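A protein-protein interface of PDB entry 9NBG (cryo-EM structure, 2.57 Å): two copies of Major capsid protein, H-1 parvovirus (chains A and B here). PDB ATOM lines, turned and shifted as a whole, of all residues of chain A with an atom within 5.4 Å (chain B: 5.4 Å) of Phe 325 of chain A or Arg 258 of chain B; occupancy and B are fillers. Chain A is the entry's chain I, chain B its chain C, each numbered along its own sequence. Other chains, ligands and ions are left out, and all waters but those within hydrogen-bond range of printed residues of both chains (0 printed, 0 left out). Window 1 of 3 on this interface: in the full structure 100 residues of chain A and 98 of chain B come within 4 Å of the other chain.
Phe 325 of chain A touches just these residues of chain B: Asn 257 (3.1 Å), Arg 258 (3.7 Å), Ala 300 (3.8 Å) and Arg 379 (3.5 Å). Arg 258 of chain B touches just these residues of chain A: Asp 70 (2.7 Å), Thr 72 (3.0 Å), Tyr 184 (3.7 Å), Gly 322 (3.7 Å), Gly 323 (3.9 Å), Pro 324 (2.6 Å) and Phe 325 (3.7 Å). Of the printed residues of chain B, Gly 322 of chain A touches Arg 258 and His 259. Of the printed residues of chain A, Arg 304 of chain B touches Tyr 184 (3.1 Å). Of the printed residues of chain B, Ala 319 of chain A touches Arg 379. Of the printed residues of chain B, Asp 70 of chain A touches Arg 258, Glu 299 and Ala 300. Of the printed residues of chain A, Ile 308 of chain B touches Asn 320 (3.99 Å).
Printed residues of chain A that touch a printed residue of chain B: Asp 70, Asp 71, Thr 72, Tyr 184, Glu 318, Ala 319, Asn 320, Gly 322, Gly 323, Pro 324, Phe 325, Lys 326 and Val 327. Hydrophobic or aromatic side chains of chain A that line the printed part of chain B: Tyr 184, Pro 324, Phe 325 and Val 327. Among the printed residues, Asp or Glu carboxylates within 4 Å of a Lys or Arg side-chain nitrogen of the other chain: Asp 70 of chain A with Arg 258 of chain B and Glu 318 of chain A with Arg 379 of chain B.
No position is printed for both chains.
The side-chain carboxylate of Glu 318 of chain A sits at hydrogen-bond distance from the side-chain amide nitrogen of Asn 316 of chain A, at 2.9 Å. OD1 of Asp 70 of chain A lies within hydrogen-bond range of OG1 of Thr 72 of chain A (2.8 Å). OG1 of Thr 256 of chain B sits close to N of Arg 258 of chain B (3.1 Å). O of Asn 316 of chain A sits close to N of Val 327 of chain A, 3.1 Å away. The side-chain carboxylate (OE2) of Glu 299 of chain B lies within salt-bridge range of the guanidinium group (NH2) of Arg 304 of chain B. The guanidinium group (NH1) of Arg 304 of chain B lies within hydrogen-bond range of the backbone carbonyl oxygen (O) of Leu 260 of chain B, at 2.8 Å.
The side-chain carboxylate (OD2) of Asp 70 of chain A is in salt-bridge range of the guanidinium group (NH1) of Arg 258 of chain B, at 2.7 Å. The side-chain carboxylate of Glu 318 of chain A is in hydrogen-bond range of the side-chain amide nitrogen of Gln 307 of chain B (2.9 Å). O of Ala 300 of chain B lies within hydrogen-bond range of N of Lys 326 of chain A (2.9 Å). The guanidinium group (NH1) of Arg 379 of chain B sits close to the side-chain amide nitrogen (ND2) of Asn 320 of chain A, 3.0 Å away. The backbone carbonyl oxygen (O) of Asp 70 of chain A is in hydrogen-bond range of the backbone NH (N) of Ala 300 of chain B (3.2 Å). OH of Tyr 184 of chain A sits close to OE2 of Glu 299 of chain B (2.4 Å). OH of Tyr 184 of chain A lies within hydrogen-bond range of NH1 of Arg 304 of chain B (3.1 Å). The side-chain carboxylate (OE2) of Glu 318 of chain A lies within salt-bridge range of the guanidinium group (NE) of Arg 379 of chain B, at 2.5 Å. The guanidinium group of Arg 258 of chain B is in hydrogen-bond range of the backbone carbonyl oxygen of Thr 72 of chain A, 3.0 Å away. NH1 of Arg 258 of chain B is in hydrogen-bond range of O of Pro 324 of chain A, at 2.6 Å. The backbone NH (N) of Glu 299 of chain B is in hydrogen-bond range of the side-chain carboxylate (OD1) of Asp 71 of chain A (2.7 Å).
Among the printed residues, merely in contact across the chains: Asp 70 of chain A with Glu 299 of chain B (3.6 Å), Tyr 184 of chain A with Arg 258 of chain B (3.7 Å), Tyr 184 of chain A with His 259 of chain B (3.5 Å), Tyr 184 of chain A with Leu 260 of chain B (3.6 Å), Ala 319 of chain A with Arg 379 of chain B (3.7 Å), Asn 320 of chain A with Thr 256 of chain B (3.7 Å), Asn 320 of chain A with Ile 308 of chain B (3.99 Å), Gly 322 of chain A with Arg 258 of chain B (3.7 Å), Gly 322 of chain A with His 259 of chain B (3.8 Å), Gly 323 of chain A with Arg 258 of chain B (3.9 Å), Pro 324 of chain A with Ala 300 of chain B (3.8 Å), Phe 325 of chain A with Asn 257 of chain B (3.1 Å), Phe 325 of chain A with Arg 258 of chain B (3.7 Å), Phe 325 of chain A with Ala 300 of chain B (3.8 Å), Phe 325 of chain A with Arg 379 of chain B (3.5 Å) and Val 327 of chain A with Gln 307 of chain B (3.9 Å).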
ATOM      1  N   ASP A  70      -0.346 -20.471 -15.219  1.00  0.00           N
ATOM      2  CA  ASP A  70      -0.446 -19.275 -14.341  1.00  0.00           C
ATOM      3  C   ASP A  70       0.123 -18.048 -15.056  1.00  0.00           C
ATOM      4  O   ASP A  70       1.333 -18.050 -15.347  1.00  0.00           O
ATOM      5  CB  ASP A  70       0.256 -19.495 -13.002  1.00  0.00           C
ATOM      6  CG  ASP A  70       0.134 -18.310 -12.061  1.00  0.00           C
ATOM      7  OD1 ASP A  70      -1.009 -17.947 -11.730  1.00  0.00           O
ATOM      8  OD2 ASP A  70       1.182 -17.759 -11.672  1.00  0.00           O
ATOM      9  N   ASP A  71      -0.708 -17.030 -15.288  1.00  0.00           N
ATOM     10  CA  ASP A  71      -0.233 -15.766 -15.915  1.00  0.00           C
ATOM     11  C   ASP A  71      -0.535 -14.607 -14.963  1.00  0.00           C
ATOM     12  O   ASP A  71      -0.557 -13.455 -15.434  1.00  0.00           O
ATOM     13  CB  ASP A  71      -0.888 -15.541 -17.279  1.00  0.00           C
ATOM     14  CG  ASP A  71      -0.414 -16.497 -18.359  1.00  0.00           C
ATOM     15  OD1 ASP A  71       0.463 -17.332 -18.064  1.00  0.00           O
ATOM     16  OD2 ASP A  71      -0.928 -16.398 -19.491  1.00  0.00           O
ATOM     17  N   THR A  72      -0.752 -14.899 -13.680  1.00  0.00           N
ATOM     18  CA  THR A  72      -1.136 -13.850 -12.701  1.00  0.00           C
ATOM     19  C   THR A  72       0.063 -12.980 -12.321  1.00  0.00           C
ATOM     20  O   THR A  72       1.156 -13.552 -12.158  1.00  0.00           O
ATOM     21  CB  THR A  72      -1.697 -14.490 -11.431  1.00  0.00           C
ATOM     22  OG1 THR A  72      -0.651 -15.329 -10.949  1.00  0.00           O
ATOM     23  CG2 THR A  72      -2.942 -15.312 -11.678  1.00  0.00           C
ATOM     24  N   HIS A  73      -0.139 -11.662 -12.238  1.00  0.00           N
ATOM     25  CA  HIS A  73       0.960 -10.726 -11.889  1.00  0.00           C
ATOM     26  C   HIS A  73       0.432  -9.293 -11.845  1.00  0.00           C
ATOM     27  O   HIS A  73      -0.669  -9.037 -12.376  1.00  0.00           O
ATOM     28  CB  HIS A  73       2.082 -10.784 -12.928  1.00  0.00           C
ATOM     29  CG  HIS A  73       1.763 -10.079 -14.203  1.00  0.00           C
ATOM     30  ND1 HIS A  73       0.723 -10.452 -15.026  1.00  0.00           N
ATOM     31  CD2 HIS A  73       2.345  -9.031 -14.793  1.00  0.00           C
ATOM     32  CE1 HIS A  73       0.688  -9.646 -16.076  1.00  0.00           C
ATOM     33  NE2 HIS A  73       1.664  -8.774 -15.953  1.00  0.00           N
ATOM     34  N   TYR A 184       6.844  -4.950 -13.702  1.00  0.00           N
ATOM     35  CA  TYR A 184       6.053  -5.710 -12.698  1.00  0.00           C
ATOM     36  C   TYR A 184       6.024  -4.977 -11.371  1.00  0.00           C
ATOM     37  O   TYR A 184       7.018  -4.306 -11.025  1.00  0.00           O
ATOM     38  CB  TYR A 184       6.642  -7.085 -12.378  1.00  0.00           C
ATOM     39  CG  TYR A 184       6.793  -8.045 -13.546  1.00  0.00           C
ATOM     40  CD1 TYR A 184       5.725  -8.818 -13.982  1.00  0.00           C
ATOM     41  CD2 TYR A 184       8.014  -8.203 -14.185  1.00  0.00           C
ATOM     42  CE1 TYR A 184       5.862  -9.700 -15.039  1.00  0.00           C
ATOM     43  CE2 TYR A 184       8.164  -9.093 -15.233  1.00  0.00           C
ATOM     44  CZ  TYR A 184       7.085  -9.836 -15.668  1.00  0.00           C
ATOM     45  OH  TYR A 184       7.249 -10.699 -16.711  1.00  0.00           O
ATOM     46  N   ASN A 316      11.454 -28.213 -13.109  1.00  0.00           N
ATOM     47  CA  ASN A 316      11.503 -27.907 -11.662  1.00  0.00           C
ATOM     48  C   ASN A 316      10.665 -26.640 -11.481  1.00  0.00           C
ATOM     49  O   ASN A 316      11.229 -25.541 -11.573  1.00  0.00           O
ATOM     50  CB  ASN A 316      12.943 -27.740 -11.173  1.00  0.00           C
ATOM     51  CG  ASN A 316      13.047 -27.535  -9.677  1.00  0.00           C
ATOM     52  OD1 ASN A 316      12.050 -27.601  -8.962  1.00  0.00           O
ATOM     53  ND2 ASN A 316      14.255 -27.300  -9.194  1.00  0.00           N
ATOM     54  N   PHE A 317       9.356 -26.800 -11.290  1.00  0.00           N
ATOM     55  CA  PHE A 317       8.481 -25.626 -11.054  1.00  0.00           C
ATOM     56  C   PHE A 317       8.624 -25.206  -9.590  1.00  0.00           C
ATOM     57  O   PHE A 317       7.884 -25.733  -8.738  1.00  0.00           O
ATOM     58  CB  PHE A 317       7.040 -25.954 -11.444  1.00  0.00           C
ATOM     59  CG  PHE A 317       6.826 -26.120 -12.926  1.00  0.00           C
ATOM     60  CD1 PHE A 317       6.898 -25.031 -13.779  1.00  0.00           C
ATOM     61  CD2 PHE A 317       6.586 -27.369 -13.473  1.00  0.00           C
ATOM     62  CE1 PHE A 317       6.707 -25.185 -15.141  1.00  0.00           C
ATOM     63  CE2 PHE A 317       6.400 -27.522 -14.836  1.00  0.00           C
ATOM     64  CZ  PHE A 317       6.462 -26.431 -15.668  1.00  0.00           C
ATOM     65  N   GLU A 318       9.559 -24.294  -9.314  1.00  0.00           N
ATOM     66  CA  GLU A 318       9.758 -23.795  -7.927  1.00  0.00           C
ATOM     67  C   GLU A 318       8.714 -22.709  -7.651  1.00  0.00           C
ATOM     68  O   GLU A 318       8.138 -22.193  -8.625  1.00  0.00           O
ATOM     69  CB  GLU A 318      11.191 -23.301  -7.741  1.00  0.00           C
ATOM     70  CG  GLU A 318      12.215 -24.418  -7.803  1.00  0.00           C
ATOM     71  CD  GLU A 318      13.648 -23.996  -7.530  1.00  0.00           C
ATOM     72  OE1 GLU A 318      14.539 -24.865  -7.596  1.00  0.00           O
ATOM     73  OE2 GLU A 318      13.870 -22.802  -7.250  1.00  0.00           O
ATOM     74  N   ALA A 319       8.484 -22.375  -6.379  1.00  0.00           N
ATOM     75  CA  ALA A 319       7.402 -21.418  -6.052  1.00  0.00           C
ATOM     76  C   ALA A 319       7.844 -20.445  -4.956  1.00  0.00           C
ATOM     77  O   ALA A 319       8.368 -20.913  -3.931  1.00  0.00           O
ATOM     78  CB  ALA A 319       6.164 -22.173  -5.639  1.00  0.00           C
ATOM     79  N   ASN A 320       7.673 -19.144  -5.186  1.00  0.00           N
ATOM     80  CA  ASN A 320       8.051 -18.129  -4.168  1.00  0.00           C
ATOM     81  C   ASN A 320       6.810 -17.321  -3.792  1.00  0.00           C
ATOM     82  O   ASN A 320       5.691 -17.821  -4.007  1.00  0.00           O
ATOM     83  CB  ASN A 320       9.158 -17.201  -4.670  1.00  0.00           C
ATOM     84  CG  ASN A 320      10.476 -17.908  -4.904  1.00  0.00           C
ATOM     85  OD1 ASN A 320      10.598 -19.106  -4.663  1.00  0.00           O
ATOM     86  ND2 ASN A 320      11.472 -17.172  -5.370  1.00  0.00           N
ATOM     87  N   GLY A 322       5.826 -15.045  -5.367  1.00  0.00           N
ATOM     88  CA  GLY A 322       5.304 -14.552  -6.656  1.00  0.00           C
ATOM     89  C   GLY A 322       4.664 -15.647  -7.489  1.00  0.00           C
ATOM     90  O   GLY A 322       4.375 -15.389  -8.673  1.00  0.00           O
ATOM     91  N   GLY A 323       4.441 -16.824  -6.903  1.00  0.00           N
ATOM     92  CA  GLY A 323       3.766 -17.918  -7.629  1.00  0.00           C
ATOM     93  C   GLY A 323       4.751 -18.902  -8.235  1.00  0.00           C
ATOM     94  O   GLY A 323       5.964 -18.740  -8.007  1.00  0.00           O
ATOM     95  N   PRO A 324       4.300 -19.935  -8.988  1.00  0.00           N
ATOM     96  CA  PRO A 324       5.208 -20.951  -9.517  1.00  0.00           C
ATOM     97  C   PRO A 324       5.942 -20.454 -10.770  1.00  0.00           C
ATOM     98  O   PRO A 324       5.439 -19.563 -11.427  1.00  0.00           O
ATOM     99  CB  PRO A 324       4.266 -22.098  -9.896  1.00  0.00           C
ATOM    100  CG  PRO A 324       2.994 -21.402 -10.311  1.00  0.00           C
ATOM    101  CD  PRO A 324       2.905 -20.207  -9.385  1.00  0.00           C
ATOM    102  N   PHE A 325       7.105 -21.040 -11.060  1.00  0.00           N
ATOM    103  CA  PHE A 325       7.895 -20.613 -12.246  1.00  0.00           C
ATOM    104  C   PHE A 325       8.743 -21.775 -12.764  1.00  0.00           C
ATOM    105  O   PHE A 325       9.308 -22.518 -11.942  1.00  0.00           O
ATOM    106  CB  PHE A 325       8.757 -19.396 -11.905  1.00  0.00           C
ATOM    107  CG  PHE A 325       9.587 -19.512 -10.652  1.00  0.00           C
ATOM    108  CD1 PHE A 325      10.840 -20.103 -10.679  1.00  0.00           C
ATOM    109  CD2 PHE A 325       9.120 -19.019  -9.443  1.00  0.00           C
ATOM    110  CE1 PHE A 325      11.602 -20.202  -9.527  1.00  0.00           C
ATOM    111  CE2 PHE A 325       9.881 -19.122  -8.292  1.00  0.00           C
ATOM    112  CZ  PHE A 325      11.123 -19.712  -8.335  1.00  0.00           C
ATOM    113  N   LYS A 326       8.853 -21.926 -14.083  1.00  0.00           N
ATOM    114  CA  LYS A 326       9.734 -22.982 -14.651  1.00  0.00           C
ATOM    115  C   LYS A 326      11.193 -22.569 -14.452  1.00  0.00           C
ATOM    116  O   LYS A 326      11.589 -21.519 -14.992  1.00  0.00           O
ATOM    117  CB  LYS A 326       9.421 -23.194 -16.134  1.00  0.00           C
ATOM    118  CG  LYS A 326      10.421 -24.044 -16.903  1.00  0.00           C
ATOM    119  CD  LYS A 326      10.548 -25.456 -16.381  1.00  0.00           C
ATOM    120  CE  LYS A 326      11.496 -26.292 -17.213  1.00  0.00           C
ATOM    121  NZ  LYS A 326      12.815 -25.630 -17.365  1.00  0.00           N
ATOM    122  N   VAL A 327      11.957 -23.362 -13.700  1.00  0.00           N
ATOM    123  CA  VAL A 327      13.392 -23.040 -13.449  1.00  0.00           C
ATOM    124  C   VAL A 327      14.144 -23.096 -14.782  1.00  0.00           C
ATOM    125  O   VAL A 327      13.981 -24.086 -15.513  1.00  0.00           O
ATOM    126  CB  VAL A 327      14.006 -23.990 -12.405  1.00  0.00           C
ATOM    127  CG1 VAL A 327      15.523 -24.039 -12.493  1.00  0.00           C
ATOM    128  CG2 VAL A 327      13.564 -23.624 -11.000  1.00  0.00           C
ATOM    129  N   THR B 256      11.273 -12.087  -7.949  1.00  0.00           N
ATOM    130  CA  THR B 256      11.453 -13.539  -8.188  1.00  0.00           C
ATOM    131  C   THR B 256      11.551 -13.740  -9.700  1.00  0.00           C
ATOM    132  O   THR B 256      11.503 -12.734 -10.430  1.00  0.00           O
ATOM    133  CB  THR B 256      10.273 -14.328  -7.616  1.00  0.00           C
ATOM    134  OG1 THR B 256       9.148 -14.098  -8.467  1.00  0.00           O
ATOM    135  CG2 THR B 256       9.935 -13.931  -6.197  1.00  0.00           C
ATOM    136  N   ASN B 257      11.713 -14.988 -10.138  1.00  0.00           N
ATOM    137  CA  ASN B 257      11.820 -15.275 -11.591  1.00  0.00           C
ATOM    138  C   ASN B 257      10.531 -14.809 -12.272  1.00  0.00           C
ATOM    139  O   ASN B 257      10.570 -14.545 -13.480  1.00  0.00           O
ATOM    140  CB  ASN B 257      12.135 -16.749 -11.848  1.00  0.00           C
ATOM    141  CG  ASN B 257      13.493 -17.151 -11.314  1.00  0.00           C
ATOM    142  OD1 ASN B 257      13.599 -18.030 -10.464  1.00  0.00           O
ATOM    143  ND2 ASN B 257      14.538 -16.501 -11.802  1.00  0.00           N
ATOM    144  N   ARG B 258       9.441 -14.687 -11.509  1.00  0.00           N
ATOM    145  CA  ARG B 258       8.134 -14.285 -12.096  1.00  0.00           C
ATOM    146  C   ARG B 258       8.070 -12.757 -12.219  1.00  0.00           C
ATOM    147  O   ARG B 258       7.032 -12.245 -12.687  1.00  0.00           O
ATOM    148  CB  ARG B 258       6.971 -14.796 -11.238  1.00  0.00           C
ATOM    149  CG  ARG B 258       6.768 -16.301 -11.327  1.00  0.00           C
ATOM    150  CD  ARG B 258       6.400 -16.720 -12.743  1.00  0.00           C
ATOM    151  NE  ARG B 258       5.088 -16.227 -13.176  1.00  0.00           N
ATOM    152  CZ  ARG B 258       3.922 -16.558 -12.631  1.00  0.00           C
ATOM    153  NH1 ARG B 258       3.854 -17.530 -11.739  1.00  0.00           N
ATOM    154  NH2 ARG B 258       2.823 -15.919 -12.988  1.00  0.00           N
ATOM    155  N   HIS B 259       9.136 -12.063 -11.817  1.00  0.00           N
ATOM    156  CA  HIS B 259       9.160 -10.579 -11.880  1.00  0.00           C
ATOM    157  C   HIS B 259      10.426 -10.129 -12.610  1.00  0.00           C
ATOM    158  O   HIS B 259      10.997  -9.085 -12.235  1.00  0.00           O
ATOM    159  CB  HIS B 259       9.125  -9.975 -10.474  1.00  0.00           C
ATOM    160  CG  HIS B 259       8.067 -10.536  -9.586  1.00  0.00           C
ATOM    161  ND1 HIS B 259       8.351 -11.124  -8.375  1.00  0.00           N
ATOM    162  CD2 HIS B 259       6.737 -10.589  -9.721  1.00  0.00           C
ATOM    163  CE1 HIS B 259       7.223 -11.522  -7.807  1.00  0.00           C
ATOM    164  NE2 HIS B 259       6.229 -11.207  -8.609  1.00  0.00           N
ATOM    165  N   LEU B 260      10.850 -10.887 -13.622  1.00  0.00           N
ATOM    166  CA  LEU B 260      12.098 -10.552 -14.355  1.00  0.00           C
ATOM    167  C   LEU B 260      11.780 -10.285 -15.827  1.00  0.00           C
ATOM    168  O   LEU B 260      11.268 -11.200 -16.487  1.00  0.00           O
ATOM    169  CB  LEU B 260      13.071 -11.730 -14.239  1.00  0.00           C
ATOM    170  CG  LEU B 260      13.719 -11.935 -12.873  1.00  0.00           C
ATOM    171  CD1 LEU B 260      14.895 -12.890 -12.989  1.00  0.00           C
ATOM    172  CD2 LEU B 260      14.165 -10.607 -12.283  1.00  0.00           C
ATOM    173  N   GLU B 299       3.091 -16.946 -18.374  1.00  0.00           N
ATOM    174  CA  GLU B 299       4.076 -16.226 -17.525  1.00  0.00           C
ATOM    175  C   GLU B 299       4.947 -17.244 -16.784  1.00  0.00           C
ATOM    176  O   GLU B 299       6.152 -16.981 -16.623  1.00  0.00           O
ATOM    177  CB  GLU B 299       3.354 -15.295 -16.551  1.00  0.00           C
ATOM    178  CG  GLU B 299       4.274 -14.305 -15.862  1.00  0.00           C
ATOM    179  CD  GLU B 299       4.839 -13.217 -16.759  1.00  0.00           C
ATOM    180  OE1 GLU B 299       4.502 -13.204 -17.959  1.00  0.00           O
ATOM    181  OE2 GLU B 299       5.619 -12.385 -16.254  1.00  0.00           O
ATOM    182  N   ALA B 300       4.355 -18.363 -16.360  1.00  0.00           N
ATOM    183  CA  ALA B 300       5.104 -19.374 -15.576  1.00  0.00           C
ATOM    184  C   ALA B 300       6.093 -20.129 -16.469  1.00  0.00           C
ATOM    185  O   ALA B 300       7.139 -20.557 -15.951  1.00  0.00           O
ATOM    186  CB  ALA B 300       4.136 -20.323 -14.919  1.00  0.00           C
ATOM    187  N   ARG B 304      13.332 -17.285 -18.342  1.00  0.00           N
ATOM    188  CA  ARG B 304      13.866 -16.150 -17.544  1.00  0.00           C
ATOM    189  C   ARG B 304      15.394 -16.165 -17.618  1.00  0.00           C
ATOM    190  O   ARG B 304      15.961 -17.245 -17.851  1.00  0.00           O
ATOM    191  CB  ARG B 304      13.388 -16.260 -16.093  1.00  0.00           C
ATOM    192  CG  ARG B 304      11.880 -16.381 -15.948  1.00  0.00           C
ATOM    193  CD  ARG B 304      11.157 -15.164 -16.489  1.00  0.00           C
ATOM    194  NE  ARG B 304       9.743 -15.233 -16.155  1.00  0.00           N
ATOM    195  CZ  ARG B 304       8.854 -14.290 -16.433  1.00  0.00           C
ATOM    196  NH1 ARG B 304       9.258 -13.091 -16.815  1.00  0.00           N
ATOM    197  NH2 ARG B 304       7.564 -14.545 -16.315  1.00  0.00           N
ATOM    198  N   GLN B 307      18.037 -18.091 -12.276  1.00  0.00           N
ATOM    199  CA  GLN B 307      17.186 -18.618 -11.179  1.00  0.00           C
ATOM    200  C   GLN B 307      17.434 -17.807  -9.904  1.00  0.00           C
ATOM    201  O   GLN B 307      18.567 -17.853  -9.393  1.00  0.00           O
ATOM    202  CB  GLN B 307      17.511 -20.089 -10.928  1.00  0.00           C
ATOM    203  CG  GLN B 307      16.610 -20.749  -9.897  1.00  0.00           C
ATOM    204  CD  GLN B 307      17.176 -22.065  -9.419  1.00  0.00           C
ATOM    205  OE1 GLN B 307      18.273 -22.464  -9.800  1.00  0.00           O
ATOM    206  NE2 GLN B 307      16.430 -22.744  -8.565  1.00  0.00           N
ATOM    207  N   ILE B 308      16.423 -17.066  -9.447  1.00  0.00           N
ATOM    208  CA  ILE B 308      16.556 -16.286  -8.184  1.00  0.00           C
ATOM    209  C   ILE B 308      16.318 -17.251  -7.021  1.00  0.00           C
ATOM    210  O   ILE B 308      15.158 -17.650  -6.817  1.00  0.00           O
ATOM    211  CB  ILE B 308      15.569 -15.103  -8.158  1.00  0.00           C
ATOM    212  CG1 ILE B 308      15.676 -14.249  -9.423  1.00  0.00           C
ATOM    213  CG2 ILE B 308      15.757 -14.274  -6.899  1.00  0.00           C
ATOM    214  CD1 ILE B 308      17.040 -13.635  -9.633  1.00  0.00           C
ATOM    215  N   ARG B 379      12.003 -20.327  -1.009  1.00  0.00           N
ATOM    216  CA  ARG B 379      11.366 -21.472  -1.711  1.00  0.00           C
ATOM    217  C   ARG B 379      10.173 -21.987  -0.891  1.00  0.00           C
ATOM    218  O   ARG B 379      10.400 -22.446   0.250  1.00  0.00           O
ATOM    219  CB  ARG B 379      12.374 -22.608  -1.910  1.00  0.00           C
ATOM    220  CG  ARG B 379      13.499 -22.269  -2.876  1.00  0.00           C
ATOM    221  CD  ARG B 379      12.925 -21.890  -4.227  1.00  0.00           C
ATOM    222  NE  ARG B 379      13.962 -21.437  -5.158  1.00  0.00           N
ATOM    223  CZ  ARG B 379      13.997 -20.233  -5.711  1.00  0.00           C
ATOM    224  NH1 ARG B 379      13.714 -19.166  -4.988  1.00  0.00           N
ATOM    225  NH2 ARG B 379      14.328 -20.102  -6.983  1.00  0.00           N
